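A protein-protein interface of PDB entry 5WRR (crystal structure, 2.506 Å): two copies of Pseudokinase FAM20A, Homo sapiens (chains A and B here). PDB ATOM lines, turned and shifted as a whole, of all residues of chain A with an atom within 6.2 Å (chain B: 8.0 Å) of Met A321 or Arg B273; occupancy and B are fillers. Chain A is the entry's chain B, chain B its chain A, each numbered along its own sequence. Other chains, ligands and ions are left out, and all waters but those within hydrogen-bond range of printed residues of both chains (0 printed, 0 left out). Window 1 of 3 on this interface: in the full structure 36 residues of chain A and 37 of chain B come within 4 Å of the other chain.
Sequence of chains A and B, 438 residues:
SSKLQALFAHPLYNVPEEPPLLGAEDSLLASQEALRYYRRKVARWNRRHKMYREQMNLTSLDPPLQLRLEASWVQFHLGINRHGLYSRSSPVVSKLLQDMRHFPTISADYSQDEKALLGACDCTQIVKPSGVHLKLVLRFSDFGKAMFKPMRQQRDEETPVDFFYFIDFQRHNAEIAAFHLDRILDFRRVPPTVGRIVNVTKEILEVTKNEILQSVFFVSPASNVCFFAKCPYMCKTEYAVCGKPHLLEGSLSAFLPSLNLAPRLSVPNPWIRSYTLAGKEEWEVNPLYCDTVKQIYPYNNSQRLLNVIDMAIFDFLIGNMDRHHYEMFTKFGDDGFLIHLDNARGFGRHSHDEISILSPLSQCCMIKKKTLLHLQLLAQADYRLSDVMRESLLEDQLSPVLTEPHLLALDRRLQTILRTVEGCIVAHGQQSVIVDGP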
ATOM      1  N   PHE A 166     -10.348 -34.081  23.585  1.00  0.00           N
ATOM      2  CA  PHE A 166     -10.981 -33.955  22.278  1.00  0.00           C
ATOM      3  C   PHE A 166     -10.389 -34.908  21.249  1.00  0.00           C
ATOM      4  O   PHE A 166     -10.864 -34.942  20.109  1.00  0.00           O
ATOM      5  CB  PHE A 166     -10.879 -32.511  21.765  1.00  0.00           C
ATOM      6  CG  PHE A 166     -11.663 -31.513  22.579  1.00  0.00           C
ATOM      7  CD1 PHE A 166     -12.592 -31.928  23.521  1.00  0.00           C
ATOM      8  CD2 PHE A 166     -11.470 -30.153  22.394  1.00  0.00           C
ATOM      9  CE1 PHE A 166     -13.309 -31.007  24.267  1.00  0.00           C
ATOM     10  CE2 PHE A 166     -12.184 -29.227  23.134  1.00  0.00           C
ATOM     11  CZ  PHE A 166     -13.104 -29.654  24.071  1.00  0.00           C
ATOM     12  N   ILE A 272     -27.613 -28.701  17.759  1.00  0.00           N
ATOM     13  CA  ILE A 272     -26.187 -28.967  17.946  1.00  0.00           C
ATOM     14  C   ILE A 272     -25.668 -28.300  19.215  1.00  0.00           C
ATOM     15  O   ILE A 272     -24.698 -28.769  19.824  1.00  0.00           O
ATOM     16  CB  ILE A 272     -25.394 -28.515  16.701  1.00  0.00           C
ATOM     17  CG1 ILE A 272     -23.910 -28.869  16.842  1.00  0.00           C
ATOM     18  CG2 ILE A 272     -25.571 -27.023  16.460  1.00  0.00           C
ATOM     19  CD1 ILE A 272     -23.658 -30.332  17.148  1.00  0.00           C
ATOM     20  N   ARG A 273     -26.299 -27.210  19.639  1.00  0.00           N
ATOM     21  CA  ARG A 273     -25.897 -26.486  20.833  1.00  0.00           C
ATOM     22  C   ARG A 273     -27.043 -26.429  21.832  1.00  0.00           C
ATOM     23  O   ARG A 273     -28.220 -26.419  21.458  1.00  0.00           O
ATOM     24  CB  ARG A 273     -25.438 -25.062  20.489  1.00  0.00           C
ATOM     25  CG  ARG A 273     -24.490 -25.009  19.311  1.00  0.00           C
ATOM     26  CD  ARG A 273     -23.202 -25.753  19.619  1.00  0.00           C
ATOM     27  NE  ARG A 273     -22.222 -24.876  20.255  1.00  0.00           N
ATOM     28  CZ  ARG A 273     -22.054 -24.761  21.567  1.00  0.00           C
ATOM     29  NH1 ARG A 273     -22.803 -25.471  22.402  1.00  0.00           N
ATOM     30  NH2 ARG A 273     -21.135 -23.933  22.042  1.00  0.00           N
ATOM     31  N   SER A 274     -26.682 -26.405  23.107  1.00  0.00           N
ATOM     32  CA  SER A 274     -27.619 -26.141  24.184  1.00  0.00           C
ATOM     33  C   SER A 274     -27.446 -24.703  24.658  1.00  0.00           C
ATOM     34  O   SER A 274     -26.427 -24.060  24.401  1.00  0.00           O
ATOM     35  CB  SER A 274     -27.402 -27.114  25.345  1.00  0.00           C
ATOM     36  OG  SER A 274     -26.053 -27.092  25.777  1.00  0.00           O
ATOM     37  N   ASP A 315     -27.544 -40.447  18.259  1.00  0.00           N
ATOM     38  CA  ASP A 315     -26.375 -39.707  18.727  1.00  0.00           C
ATOM     39  C   ASP A 315     -26.222 -39.808  20.240  1.00  0.00           C
ATOM     40  O   ASP A 315     -25.099 -39.875  20.755  1.00  0.00           O
ATOM     41  CB  ASP A 315     -26.471 -38.246  18.298  1.00  0.00           C
ATOM     42  CG  ASP A 315     -26.295 -38.063  16.806  1.00  0.00           C
ATOM     43  OD1 ASP A 315     -25.576 -38.870  16.180  1.00  0.00           O
ATOM     44  OD2 ASP A 315     -26.886 -37.108  16.262  1.00  0.00           O
ATOM     45  N   GLY A 319     -23.142 -41.288  22.221  1.00  0.00           N
ATOM     46  CA  GLY A 319     -22.494 -40.146  22.843  1.00  0.00           C
ATOM     47  C   GLY A 319     -21.753 -39.252  21.870  1.00  0.00           C
ATOM     48  O   GLY A 319     -20.591 -38.902  22.097  1.00  0.00           O
ATOM     49  N   ASN A 320     -22.416 -38.876  20.780  1.00  0.00           N
ATOM     50  CA  ASN A 320     -21.824 -38.046  19.738  1.00  0.00           C
ATOM     51  C   ASN A 320     -22.378 -36.631  19.863  1.00  0.00           C
ATOM     52  O   ASN A 320     -23.539 -36.381  19.524  1.00  0.00           O
ATOM     53  CB  ASN A 320     -22.110 -38.627  18.356  1.00  0.00           C
ATOM     54  CG  ASN A 320     -21.632 -37.730  17.236  1.00  0.00           C
ATOM     55  OD1 ASN A 320     -20.640 -37.013  17.379  1.00  0.00           O
ATOM     56  ND2 ASN A 320     -22.339 -37.757  16.113  1.00  0.00           N
ATOM     57  N   MET A 321     -21.552 -35.713  20.358  1.00  0.00           N
ATOM     58  CA  MET A 321     -21.919 -34.309  20.483  1.00  0.00           C
ATOM     59  C   MET A 321     -21.570 -33.486  19.249  1.00  0.00           C
ATOM     60  O   MET A 321     -21.745 -32.265  19.268  1.00  0.00           O
ATOM     61  CB  MET A 321     -21.242 -33.694  21.709  1.00  0.00           C
ATOM     62  CG  MET A 321     -21.795 -34.178  23.033  1.00  0.00           C
ATOM     63  SD  MET A 321     -20.854 -33.546  24.431  1.00  0.00           S
ATOM     64  CE  MET A 321     -21.202 -31.789  24.322  1.00  0.00           C
ATOM     65  N   ASP A 322     -21.096 -34.118  18.176  1.00  0.00           N
ATOM     66  CA  ASP A 322     -20.514 -33.405  17.044  1.00  0.00           C
ATOM     67  C   ASP A 322     -21.321 -33.575  15.760  1.00  0.00           C
ATOM     68  O   ASP A 322     -20.759 -33.543  14.663  1.00  0.00           O
ATOM     69  CB  ASP A 322     -19.066 -33.837  16.826  1.00  0.00           C
ATOM     70  CG  ASP A 322     -18.136 -33.311  17.901  1.00  0.00           C
ATOM     71  OD1 ASP A 322     -17.818 -32.102  17.863  1.00  0.00           O
ATOM     72  OD2 ASP A 322     -17.722 -34.097  18.778  1.00  0.00           O
ATOM     73  N   ARG A 323     -22.636 -33.762  15.872  1.00  0.00           N
ATOM     74  CA  ARG A 323     -23.498 -33.810  14.689  1.00  0.00           C
ATOM     75  C   ARG A 323     -23.953 -32.391  14.342  1.00  0.00           C
ATOM     76  O   ARG A 323     -25.111 -32.000  14.517  1.00  0.00           O
ATOM     77  CB  ARG A 323     -24.677 -34.746  14.914  1.00  0.00           C
ATOM     78  CG  ARG A 323     -25.504 -35.000  13.657  1.00  0.00           C
ATOM     79  CD  ARG A 323     -25.757 -36.480  13.453  1.00  0.00           C
ATOM     80  NE  ARG A 323     -24.680 -37.127  12.715  1.00  0.00           N
ATOM     81  CZ  ARG A 323     -24.365 -38.412  12.831  1.00  0.00           C
ATOM     82  NH1 ARG A 323     -25.042 -39.188  13.665  1.00  0.00           N
ATOM     83  NH2 ARG A 323     -23.370 -38.919  12.118  1.00  0.00           N
ATOM     84  N   HIS A 324     -22.995 -31.611  13.837  1.00  0.00           N
ATOM     85  CA  HIS A 324     -23.288 -30.236  13.448  1.00  0.00           C
ATOM     86  C   HIS A 324     -24.224 -30.177  12.249  1.00  0.00           C
ATOM     87  O   HIS A 324     -25.020 -29.240  12.131  1.00  0.00           O
ATOM     88  CB  HIS A 324     -21.989 -29.488  13.141  1.00  0.00           C
ATOM     89  CG  HIS A 324     -20.996 -29.521  14.261  1.00  0.00           C
ATOM     90  ND1 HIS A 324     -20.085 -30.543  14.419  1.00  0.00           N
ATOM     91  CD2 HIS A 324     -20.773 -28.657  15.281  1.00  0.00           C
ATOM     92  CE1 HIS A 324     -19.342 -30.307  15.486  1.00  0.00           C
ATOM     93  NE2 HIS A 324     -19.739 -29.169  16.027  1.00  0.00           N
ATOM     94  N   ARG A 345     -16.746 -39.473  16.074  1.00  0.00           N
ATOM     95  CA  ARG A 345     -16.713 -38.819  17.377  1.00  0.00           C
ATOM     96  C   ARG A 345     -17.558 -39.535  18.427  1.00  0.00           C
ATOM     97  O   ARG A 345     -17.676 -39.039  19.553  1.00  0.00           O
ATOM     98  CB  ARG A 345     -17.168 -37.363  17.249  1.00  0.00           C
ATOM     99  CG  ARG A 345     -16.550 -36.611  16.082  1.00  0.00           C
ATOM    100  CD  ARG A 345     -15.170 -36.086  16.425  1.00  0.00           C
ATOM    101  NE  ARG A 345     -15.166 -35.366  17.695  1.00  0.00           N
ATOM    102  CZ  ARG A 345     -14.065 -34.961  18.320  1.00  0.00           C
ATOM    103  NH1 ARG A 345     -12.872 -35.202  17.790  1.00  0.00           N
ATOM    104  NH2 ARG A 345     -14.156 -34.316  19.476  1.00  0.00           N
ATOM    105  N   ARG A 349     -16.623 -41.686  25.543  1.00  0.00           N
ATOM    106  CA  ARG A 349     -16.734 -41.621  27.002  1.00  0.00           C
ATOM    107  C   ARG A 349     -17.807 -42.615  27.431  1.00  0.00           C
ATOM    108  O   ARG A 349     -19.001 -42.342  27.286  1.00  0.00           O
ATOM    109  CB  ARG A 349     -17.074 -40.218  27.493  1.00  0.00           C
ATOM    110  CG  ARG A 349     -15.993 -39.174  27.297  1.00  0.00           C
ATOM    111  CD  ARG A 349     -16.388 -37.880  27.997  1.00  0.00           C
ATOM    112  NE  ARG A 349     -15.615 -36.729  27.541  1.00  0.00           N
ATOM    113  CZ  ARG A 349     -15.995 -35.919  26.559  1.00  0.00           C
ATOM    114  NH1 ARG A 349     -17.141 -36.134  25.924  1.00  0.00           N
ATOM    115  NH2 ARG A 349     -15.231 -34.891  26.210  1.00  0.00           N
ATOM    116  N   HIS A 352     -19.907 -41.215  30.804  1.00  0.00           N
ATOM    117  CA  HIS A 352     -20.685 -39.984  30.805  1.00  0.00           C
ATOM    118  C   HIS A 352     -21.809 -40.070  29.782  1.00  0.00           C
ATOM    119  O   HIS A 352     -21.615 -40.580  28.676  1.00  0.00           O
ATOM    120  CB  HIS A 352     -19.807 -38.763  30.502  1.00  0.00           C
ATOM    121  CG  HIS A 352     -20.559 -37.468  30.495  1.00  0.00           C
ATOM    122  ND1 HIS A 352     -20.977 -36.843  31.651  1.00  0.00           N
ATOM    123  CD2 HIS A 352     -20.975 -36.684  29.473  1.00  0.00           C
ATOM    124  CE1 HIS A 352     -21.614 -35.729  31.341  1.00  0.00           C
ATOM    125  NE2 HIS A 352     -21.627 -35.607  30.026  1.00  0.00           N
ATOM    126  N   GLU A 354     -24.483 -37.539  27.881  1.00  0.00           N
ATOM    127  CA  GLU A 354     -24.815 -36.144  27.595  1.00  0.00           C
ATOM    128  C   GLU A 354     -26.275 -36.071  27.167  1.00  0.00           C
ATOM    129  O   GLU A 354     -26.607 -36.213  25.990  1.00  0.00           O
ATOM    130  CB  GLU A 354     -23.884 -35.576  26.532  1.00  0.00           C
ATOM    131  CG  GLU A 354     -23.945 -34.063  26.427  1.00  0.00           C
ATOM    132  CD  GLU A 354     -24.168 -33.400  27.773  1.00  0.00           C
ATOM    133  OE1 GLU A 354     -25.279 -32.877  28.002  1.00  0.00           O
ATOM    134  OE2 GLU A 354     -23.239 -33.424  28.608  1.00  0.00           O
ATOM    135  N   SER A 356     -28.166 -33.621  26.862  1.00  0.00           N
ATOM    136  CA  SER A 356     -28.487 -32.514  25.969  1.00  0.00           C
ATOM    137  C   SER A 356     -28.600 -32.963  24.517  1.00  0.00           C
ATOM    138  O   SER A 356     -29.252 -32.282  23.718  1.00  0.00           O
ATOM    139  CB  SER A 356     -27.438 -31.407  26.099  1.00  0.00           C
ATOM    140  OG  SER A 356     -26.185 -31.830  25.595  1.00  0.00           O
ATOM    141  N   ILE A 357     -27.969 -34.084  24.155  1.00  0.00           N
ATOM    142  CA  ILE A 357     -28.145 -34.639  22.816  1.00  0.00           C
ATOM    143  C   ILE A 357     -29.594 -35.058  22.594  1.00  0.00           C
ATOM    144  O   ILE A 357     -30.123 -34.936  21.483  1.00  0.00           O
ATOM    145  CB  ILE A 357     -27.176 -35.816  22.595  1.00  0.00           C
ATOM    146  CG1 ILE A 357     -25.732 -35.365  22.827  1.00  0.00           C
ATOM    147  CG2 ILE A 357     -27.326 -36.371  21.190  1.00  0.00           C
ATOM    148  CD1 ILE A 357     -24.737 -36.504  22.851  1.00  0.00           C
ATOM    149  N   ASN B 269     -10.313 -24.715  21.829  1.00  0.00           N
ATOM    150  CA  ASN B 269     -10.836 -24.112  23.049  1.00  0.00           C
ATOM    151  C   ASN B 269     -11.394 -25.202  23.955  1.00  0.00           C
ATOM    152  O   ASN B 269     -12.433 -25.798  23.642  1.00  0.00           O
ATOM    153  CB  ASN B 269     -11.909 -23.073  22.707  1.00  0.00           C
ATOM    154  CG  ASN B 269     -12.566 -22.468  23.939  1.00  0.00           C
ATOM    155  OD1 ASN B 269     -12.083 -22.621  25.062  1.00  0.00           O
ATOM    156  ND2 ASN B 269     -13.677 -21.772  23.729  1.00  0.00           N
ATOM    157  N   PRO B 270     -10.744 -25.486  25.089  1.00  0.00           N
ATOM    158  CA  PRO B 270     -11.217 -26.575  25.963  1.00  0.00           C
ATOM    159  C   PRO B 270     -12.604 -26.349  26.546  1.00  0.00           C
ATOM    160  O   PRO B 270     -13.178 -27.294  27.102  1.00  0.00           O
ATOM    161  CB  PRO B 270     -10.153 -26.626  27.071  1.00  0.00           C
ATOM    162  CG  PRO B 270      -8.954 -25.938  26.492  1.00  0.00           C
ATOM    163  CD  PRO B 270      -9.499 -24.878  25.586  1.00  0.00           C
ATOM    164  N   TRP B 271     -13.154 -25.139  26.448  1.00  0.00           N
ATOM    165  CA  TRP B 271     -14.475 -24.831  26.981  1.00  0.00           C
ATOM    166  C   TRP B 271     -15.486 -24.530  25.879  1.00  0.00           C
ATOM    167  O   TRP B 271     -16.533 -23.934  26.149  1.00  0.00           O
ATOM    168  CB  TRP B 271     -14.387 -23.652  27.955  1.00  0.00           C
ATOM    169  CG  TRP B 271     -13.741 -24.000  29.262  1.00  0.00           C
ATOM    170  CD1 TRP B 271     -14.356 -24.504  30.373  1.00  0.00           C
ATOM    171  CD2 TRP B 271     -12.353 -23.879  29.594  1.00  0.00           C
ATOM    172  NE1 TRP B 271     -13.439 -24.704  31.373  1.00  0.00           N
ATOM    173  CE2 TRP B 271     -12.201 -24.325  30.923  1.00  0.00           C
ATOM    174  CE3 TRP B 271     -11.224 -23.432  28.899  1.00  0.00           C
ATOM    175  CZ2 TRP B 271     -10.966 -24.338  31.572  1.00  0.00           C
ATOM    176  CZ3 TRP B 271      -9.997 -23.446  29.546  1.00  0.00           C
ATOM    177  CH2 TRP B 271      -9.880 -23.895  30.868  1.00  0.00           C
ATOM    178  N   ILE B 272     -15.198 -24.941  24.640  1.00  0.00           N
ATOM    179  CA  ILE B 272     -16.131 -24.690  23.542  1.00  0.00           C
ATOM    180  C   ILE B 272     -17.460 -25.391  23.792  1.00  0.00           C
ATOM    181  O   ILE B 272     -18.511 -24.933  23.330  1.00  0.00           O
ATOM    182  CB  ILE B 272     -15.504 -25.117  22.197  1.00  0.00           C
ATOM    183  CG1 ILE B 272     -16.429 -24.763  21.028  1.00  0.00           C
ATOM    184  CG2 ILE B 272     -15.198 -26.606  22.187  1.00  0.00           C
ATOM    185  CD1 ILE B 272     -16.839 -23.307  20.990  1.00  0.00           C
ATOM    186  N   ARG B 273     -17.447 -26.488  24.546  1.00  0.00           N
ATOM    187  CA  ARG B 273     -18.657 -27.231  24.851  1.00  0.00           C
ATOM    188  C   ARG B 273     -18.868 -27.279  26.356  1.00  0.00           C
ATOM    189  O   ARG B 273     -17.910 -27.325  27.134  1.00  0.00           O
ATOM    190  CB  ARG B 273     -18.586 -28.662  24.298  1.00  0.00           C
ATOM    191  CG  ARG B 273     -18.038 -28.752  22.885  1.00  0.00           C
ATOM    192  CD  ARG B 273     -18.902 -27.983  21.901  1.00  0.00           C
ATOM    193  NE  ARG B 273     -20.004 -28.788  21.388  1.00  0.00           N
ATOM    194  CZ  ARG B 273     -21.230 -28.781  21.899  1.00  0.00           C
ATOM    195  NH1 ARG B 273     -21.514 -28.004  22.939  1.00  0.00           N
ATOM    196  NH2 ARG B 273     -22.170 -29.549  21.361  1.00  0.00           N
ATOM    197  N   SER B 274     -20.133 -27.282  26.757  1.00  0.00           N
ATOM    198  CA  SER B 274     -20.525 -27.530  28.134  1.00  0.00           C
ATOM    199  C   SER B 274     -21.042 -28.958  28.266  1.00  0.00           C
ATOM    200  O   SER B 274     -21.385 -29.612  27.278  1.00  0.00           O
ATOM    201  CB  SER B 274     -21.591 -26.533  28.591  1.00  0.00           C
ATOM    202  OG  SER B 274     -22.703 -26.535  27.713  1.00  0.00           O
ATOM    203  N   TYR B 275     -21.091 -29.442  29.504  1.00  0.00           N
ATOM    204  CA  TYR B 275     -21.483 -30.817  29.767  1.00  0.00           C
ATOM    205  C   TYR B 275     -22.465 -30.857  30.926  1.00  0.00           C
ATOM    206  O   TYR B 275     -22.357 -30.068  31.869  1.00  0.00           O
ATOM    207  CB  TYR B 275     -20.260 -31.693  30.066  1.00  0.00           C
ATOM    208  CG  TYR B 275     -19.203 -31.629  28.985  1.00  0.00           C
ATOM    209  CD1 TYR B 275     -18.189 -30.681  29.034  1.00  0.00           C
ATOM    210  CD2 TYR B 275     -19.230 -32.503  27.906  1.00  0.00           C
ATOM    211  CE1 TYR B 275     -17.225 -30.612  28.045  1.00  0.00           C
ATOM    212  CE2 TYR B 275     -18.270 -32.443  26.912  1.00  0.00           C
ATOM    213  CZ  TYR B 275     -17.271 -31.495  26.987  1.00  0.00           C
ATOM    214  OH  TYR B 275     -16.314 -31.431  25.999  1.00  0.00           O
ATOM    215  N   THR B 276     -23.426 -31.773  30.843  1.00  0.00           N
ATOM    216  CA  THR B 276     -24.430 -31.943  31.892  1.00  0.00           C
ATOM    217  C   THR B 276     -23.862 -32.850  32.974  1.00  0.00           C
ATOM    218  O   THR B 276     -23.793 -34.069  32.810  1.00  0.00           O
ATOM    219  CB  THR B 276     -25.721 -32.515  31.317  1.00  0.00           C
ATOM    220  OG1 THR B 276     -26.253 -31.617  30.335  1.00  0.00           O
ATOM    221  CG2 THR B 276     -26.748 -32.716  32.421  1.00  0.00           C
ATOM    222  N   TRP B 283     -22.458 -26.954  35.628  1.00  0.00           N
ATOM    223  CA  TRP B 283     -21.198 -27.101  34.905  1.00  0.00           C
ATOM    224  C   TRP B 283     -20.295 -25.884  35.083  1.00  0.00           C
ATOM    225  O   TRP B 283     -19.103 -26.022  35.385  1.00  0.00           O
ATOM    226  CB  TRP B 283     -21.491 -27.340  33.425  1.00  0.00           C
ATOM    227  CG  TRP B 283     -20.360 -26.995  32.515  1.00  0.00           C
ATOM    228  CD1 TRP B 283     -20.246 -25.879  31.737  1.00  0.00           C
ATOM    229  CD2 TRP B 283     -19.179 -27.770  32.281  1.00  0.00           C
ATOM    230  NE1 TRP B 283     -19.067 -25.912  31.032  1.00  0.00           N
ATOM    231  CE2 TRP B 283     -18.393 -27.063  31.349  1.00  0.00           C
ATOM    232  CE3 TRP B 283     -18.709 -28.994  32.770  1.00  0.00           C
ATOM    233  CZ2 TRP B 283     -17.165 -27.538  30.896  1.00  0.00           C
ATOM    234  CZ3 TRP B 283     -17.490 -29.463  32.320  1.00  0.00           C
ATOM    235  CH2 TRP B 283     -16.731 -28.737  31.393  1.00  0.00           C
ATOM    236  N   TYR B 289     -13.417 -29.662  36.387  1.00  0.00           N
ATOM    237  CA  TYR B 289     -12.895 -29.635  35.023  1.00  0.00           C
ATOM    238  C   TYR B 289     -11.658 -28.749  34.915  1.00  0.00           C
ATOM    239  O   TYR B 289     -10.626 -29.170  34.376  1.00  0.00           O
ATOM    240  CB  TYR B 289     -13.980 -29.168  34.054  1.00  0.00           C
ATOM    241  CG  TYR B 289     -13.566 -29.228  32.599  1.00  0.00           C
ATOM    242  CD1 TYR B 289     -13.277 -30.440  31.990  1.00  0.00           C
ATOM    243  CD2 TYR B 289     -13.472 -28.072  31.834  1.00  0.00           C
ATOM    244  CE1 TYR B 289     -12.902 -30.500  30.658  1.00  0.00           C
ATOM    245  CE2 TYR B 289     -13.101 -28.122  30.504  1.00  0.00           C
ATOM    246  CZ  TYR B 289     -12.817 -29.338  29.921  1.00  0.00           C
ATOM    247  OH  TYR B 289     -12.448 -29.385  28.595  1.00  0.00           O
ATOM    248  N   MET B 321     -20.648 -17.886  20.780  1.00  0.00           N
ATOM    249  CA  MET B 321     -20.585 -19.296  21.142  1.00  0.00           C
ATOM    250  C   MET B 321     -19.729 -20.115  20.188  1.00  0.00           C
ATOM    251  O   MET B 321     -19.686 -21.342  20.314  1.00  0.00           O
ATOM    252  CB  MET B 321     -21.996 -19.893  21.190  1.00  0.00           C
ATOM    253  CG  MET B 321     -22.851 -19.409  22.344  1.00  0.00           C
ATOM    254  SD  MET B 321     -24.535 -20.041  22.235  1.00  0.00           S
ATOM    255  CE  MET B 321     -24.280 -21.801  22.488  1.00  0.00           C
ATOM    256  N   ARG B 323     -16.291 -19.835  19.316  1.00  0.00           N
ATOM    257  CA  ARG B 323     -14.832 -19.782  19.406  1.00  0.00           C
ATOM    258  C   ARG B 323     -14.298 -21.198  19.618  1.00  0.00           C
ATOM    259  O   ARG B 323     -13.835 -21.586  20.692  1.00  0.00           O
ATOM    260  CB  ARG B 323     -14.390 -18.830  20.510  1.00  0.00           C
ATOM    261  CG  ARG B 323     -12.892 -18.555  20.514  1.00  0.00           C
ATOM    262  CD  ARG B 323     -12.612 -17.065  20.596  1.00  0.00           C
ATOM    263  NE  ARG B 323     -12.591 -16.422  19.286  1.00  0.00           N
ATOM    264  CZ  ARG B 323     -12.886 -15.144  19.076  1.00  0.00           C
ATOM    265  NH1 ARG B 323     -13.236 -14.368  20.092  1.00  0.00           N
ATOM    266  NH2 ARG B 323     -12.838 -14.642  17.851  1.00  0.00           N
ATOM    267  N   HIS B 324     -14.393 -21.984  18.544  1.00  0.00           N
ATOM    268  CA  HIS B 324     -13.917 -23.363  18.582  1.00  0.00           C
ATOM    269  C   HIS B 324     -12.403 -23.430  18.715  1.00  0.00           C
ATOM    270  O   HIS B 324     -11.875 -24.392  19.283  1.00  0.00           O
ATOM    271  CB  HIS B 324     -14.377 -24.108  17.329  1.00  0.00           C
ATOM    272  CG  HIS B 324     -15.855 -24.053  17.102  1.00  0.00           C
ATOM    273  ND1 HIS B 324     -16.718 -25.019  17.574  1.00  0.00           N
ATOM    274  CD2 HIS B 324     -16.624 -23.145  16.455  1.00  0.00           C
ATOM    275  CE1 HIS B 324     -17.955 -24.709  17.226  1.00  0.00           C
ATOM    276  NE2 HIS B 324     -17.926 -23.577  16.547  1.00  0.00           N
ATOM    277  N   SER B 356     -22.475 -20.085  29.874  1.00  0.00           N
ATOM    278  CA  SER B 356     -21.522 -21.164  29.643  1.00  0.00           C
ATOM    279  C   SER B 356     -20.269 -20.670  28.931  1.00  0.00           C
ATOM    280  O   SER B 356     -19.213 -21.300  29.044  1.00  0.00           O
ATOM    281  CB  SER B 356     -22.174 -22.287  28.836  1.00  0.00           C
ATOM    282  OG  SER B 356     -22.451 -21.869  27.511  1.00  0.00           O
ATOM    283  N   SER B 359     -17.559 -19.964  31.351  1.00  0.00           N
ATOM    284  CA  SER B 359     -17.132 -21.110  32.151  1.00  0.00           C
ATOM    285  C   SER B 359     -15.663 -21.091  32.562  1.00  0.00           C
ATOM    286  O   SER B 359     -15.373 -21.494  33.700  1.00  0.00           O
ATOM    287  CB  SER B 359     -17.452 -22.413  31.403  1.00  0.00           C
ATOM    288  OG  SER B 359     -18.843 -22.678  31.430  1.00  0.00           O
ATOM    289  N   GLN B 363     -15.178 -21.413  36.568  1.00  0.00           N
ATOM    290  CA  GLN B 363     -14.609 -22.668  37.051  1.00  0.00           C
ATOM    291  C   GLN B 363     -13.225 -22.473  37.661  1.00  0.00           C
ATOM    292  O   GLN B 363     -12.945 -22.989  38.746  1.00  0.00           O
ATOM    293  CB  GLN B 363     -14.533 -23.696  35.917  1.00  0.00           C
ATOM    294  CG  GLN B 363     -15.876 -24.209  35.433  1.00  0.00           C
ATOM    295  CD  GLN B 363     -15.735 -25.277  34.363  1.00  0.00           C
ATOM    296  OE1 GLN B 363     -14.629 -25.578  33.911  1.00  0.00           O
ATOM    297  NE2 GLN B 363     -16.857 -25.862  33.959  1.00  0.00           N
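The guanidinium group (NH2) of Arg B273 lies within hydrogen-bond range of the backbone carbonyl oxygen (O) of Ile A272 (3.1 Å). The backbone NH of Thr B276 is in hydrogen-bond range of the side-chain carboxylate of Glu A354. NH1 of Arg A273 lies close to NH1 of Arg B273, at 2.9 Å. O of Ile B272 lies within hydrogen-bond range of NH2 of Arg A273, at 3.1 Å. NH2 of Arg B273 sits at hydrogen-bond distance from O of Met A321 (3.5 Å). The backbone carbonyl oxygen of Met B321 sits at hydrogen-bond distance from the guanidinium group of Arg A273, 3.4 Å away.
The side-chain amide oxygen (OD1) of Asn B269 lies close to the backbone NH (N) of Trp B271 (3.1 Å). The backbone carbonyl oxygen of Phe A166 lies within hydrogen-bond range of the guanidinium group of Arg A345 (3.1 Å). ND2 of Asn B269 lies within hydrogen-bond range of O of Arg B323, at 3.0 Å. The backbone carbonyl oxygen of Pro B270 is in hydrogen-bond range of the side-chain hydroxyl of Tyr B289 (2.7 Å). OE2 of Glu A354 is in hydrogen-bond range of NE2 of His A352, at 3.1 Å. N of Asn B269 is in hydrogen-bond range of O of His B324 (3.0 Å).
Among the printed residues, pairs that only touch across the chains: Phe A166 with Asn B269 (3.5 Å), Phe A166 with Pro B270 (3.8 Å), Phe A166 with Tyr B275 (3.5 Å), Ser A274 with Ser B274 (3.9 Å), Ser A274 with Met B321 (3.7 Å), Met A321 with Ser B274 (3.7 Å), Met A321 with Tyr B275 (3.7 Å), Arg A349 with Tyr B275 (3.6 Å), His A352 with Thr B276 (3.1 Å) and Glu A354 with Tyr B275 (3.4 Å).
Met A321 touches just these residues of chain B: Arg B273, Ser B274 and Tyr B275. Arg B273 touches just these residues of chain A: Ile A272, Arg A273 and Met A321. Printed residues of chain B within 4 Å of Glu A354: Tyr B275 and Thr B276. Printed residues of chain B within 4 Å of Arg A273: Ile B272, Arg B273 and Met B321. Printed residues of chain A within 4 Å of Tyr B275: Phe A166, Met A321, Arg A349 and Glu A354. Asp A315 touches none of the printed residues of chain B. The nearest residue of chain B that does not touch Met A321 is Thr B276 (6.9 Å). The nearest residue of chain A that does not touch Arg B273 is Phe A166 (5.2 Å). The nearest printed residue of chain A that does not touch Met B321 is Ile A272 (7.4 Å).
Of the 16 printed residues of chain B, 8 touch a printed residue of chain A. Among the printed residues, 16 pairs touch across the chains.
Ile A272 touches Arg B273, and with the chains exchanged Arg A273 touches Ile B272. Arg A273 touches its own counterpart, Arg B273. Ser B274 touches its own counterpart, Ser A274. Ser A274 touches Met B321, and with the chains exchanged Met A321 touches Ser B274. Of the 16 pairs that touch across the chains among the printed residues, 8 have their exchanged pair printed and touching as well.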
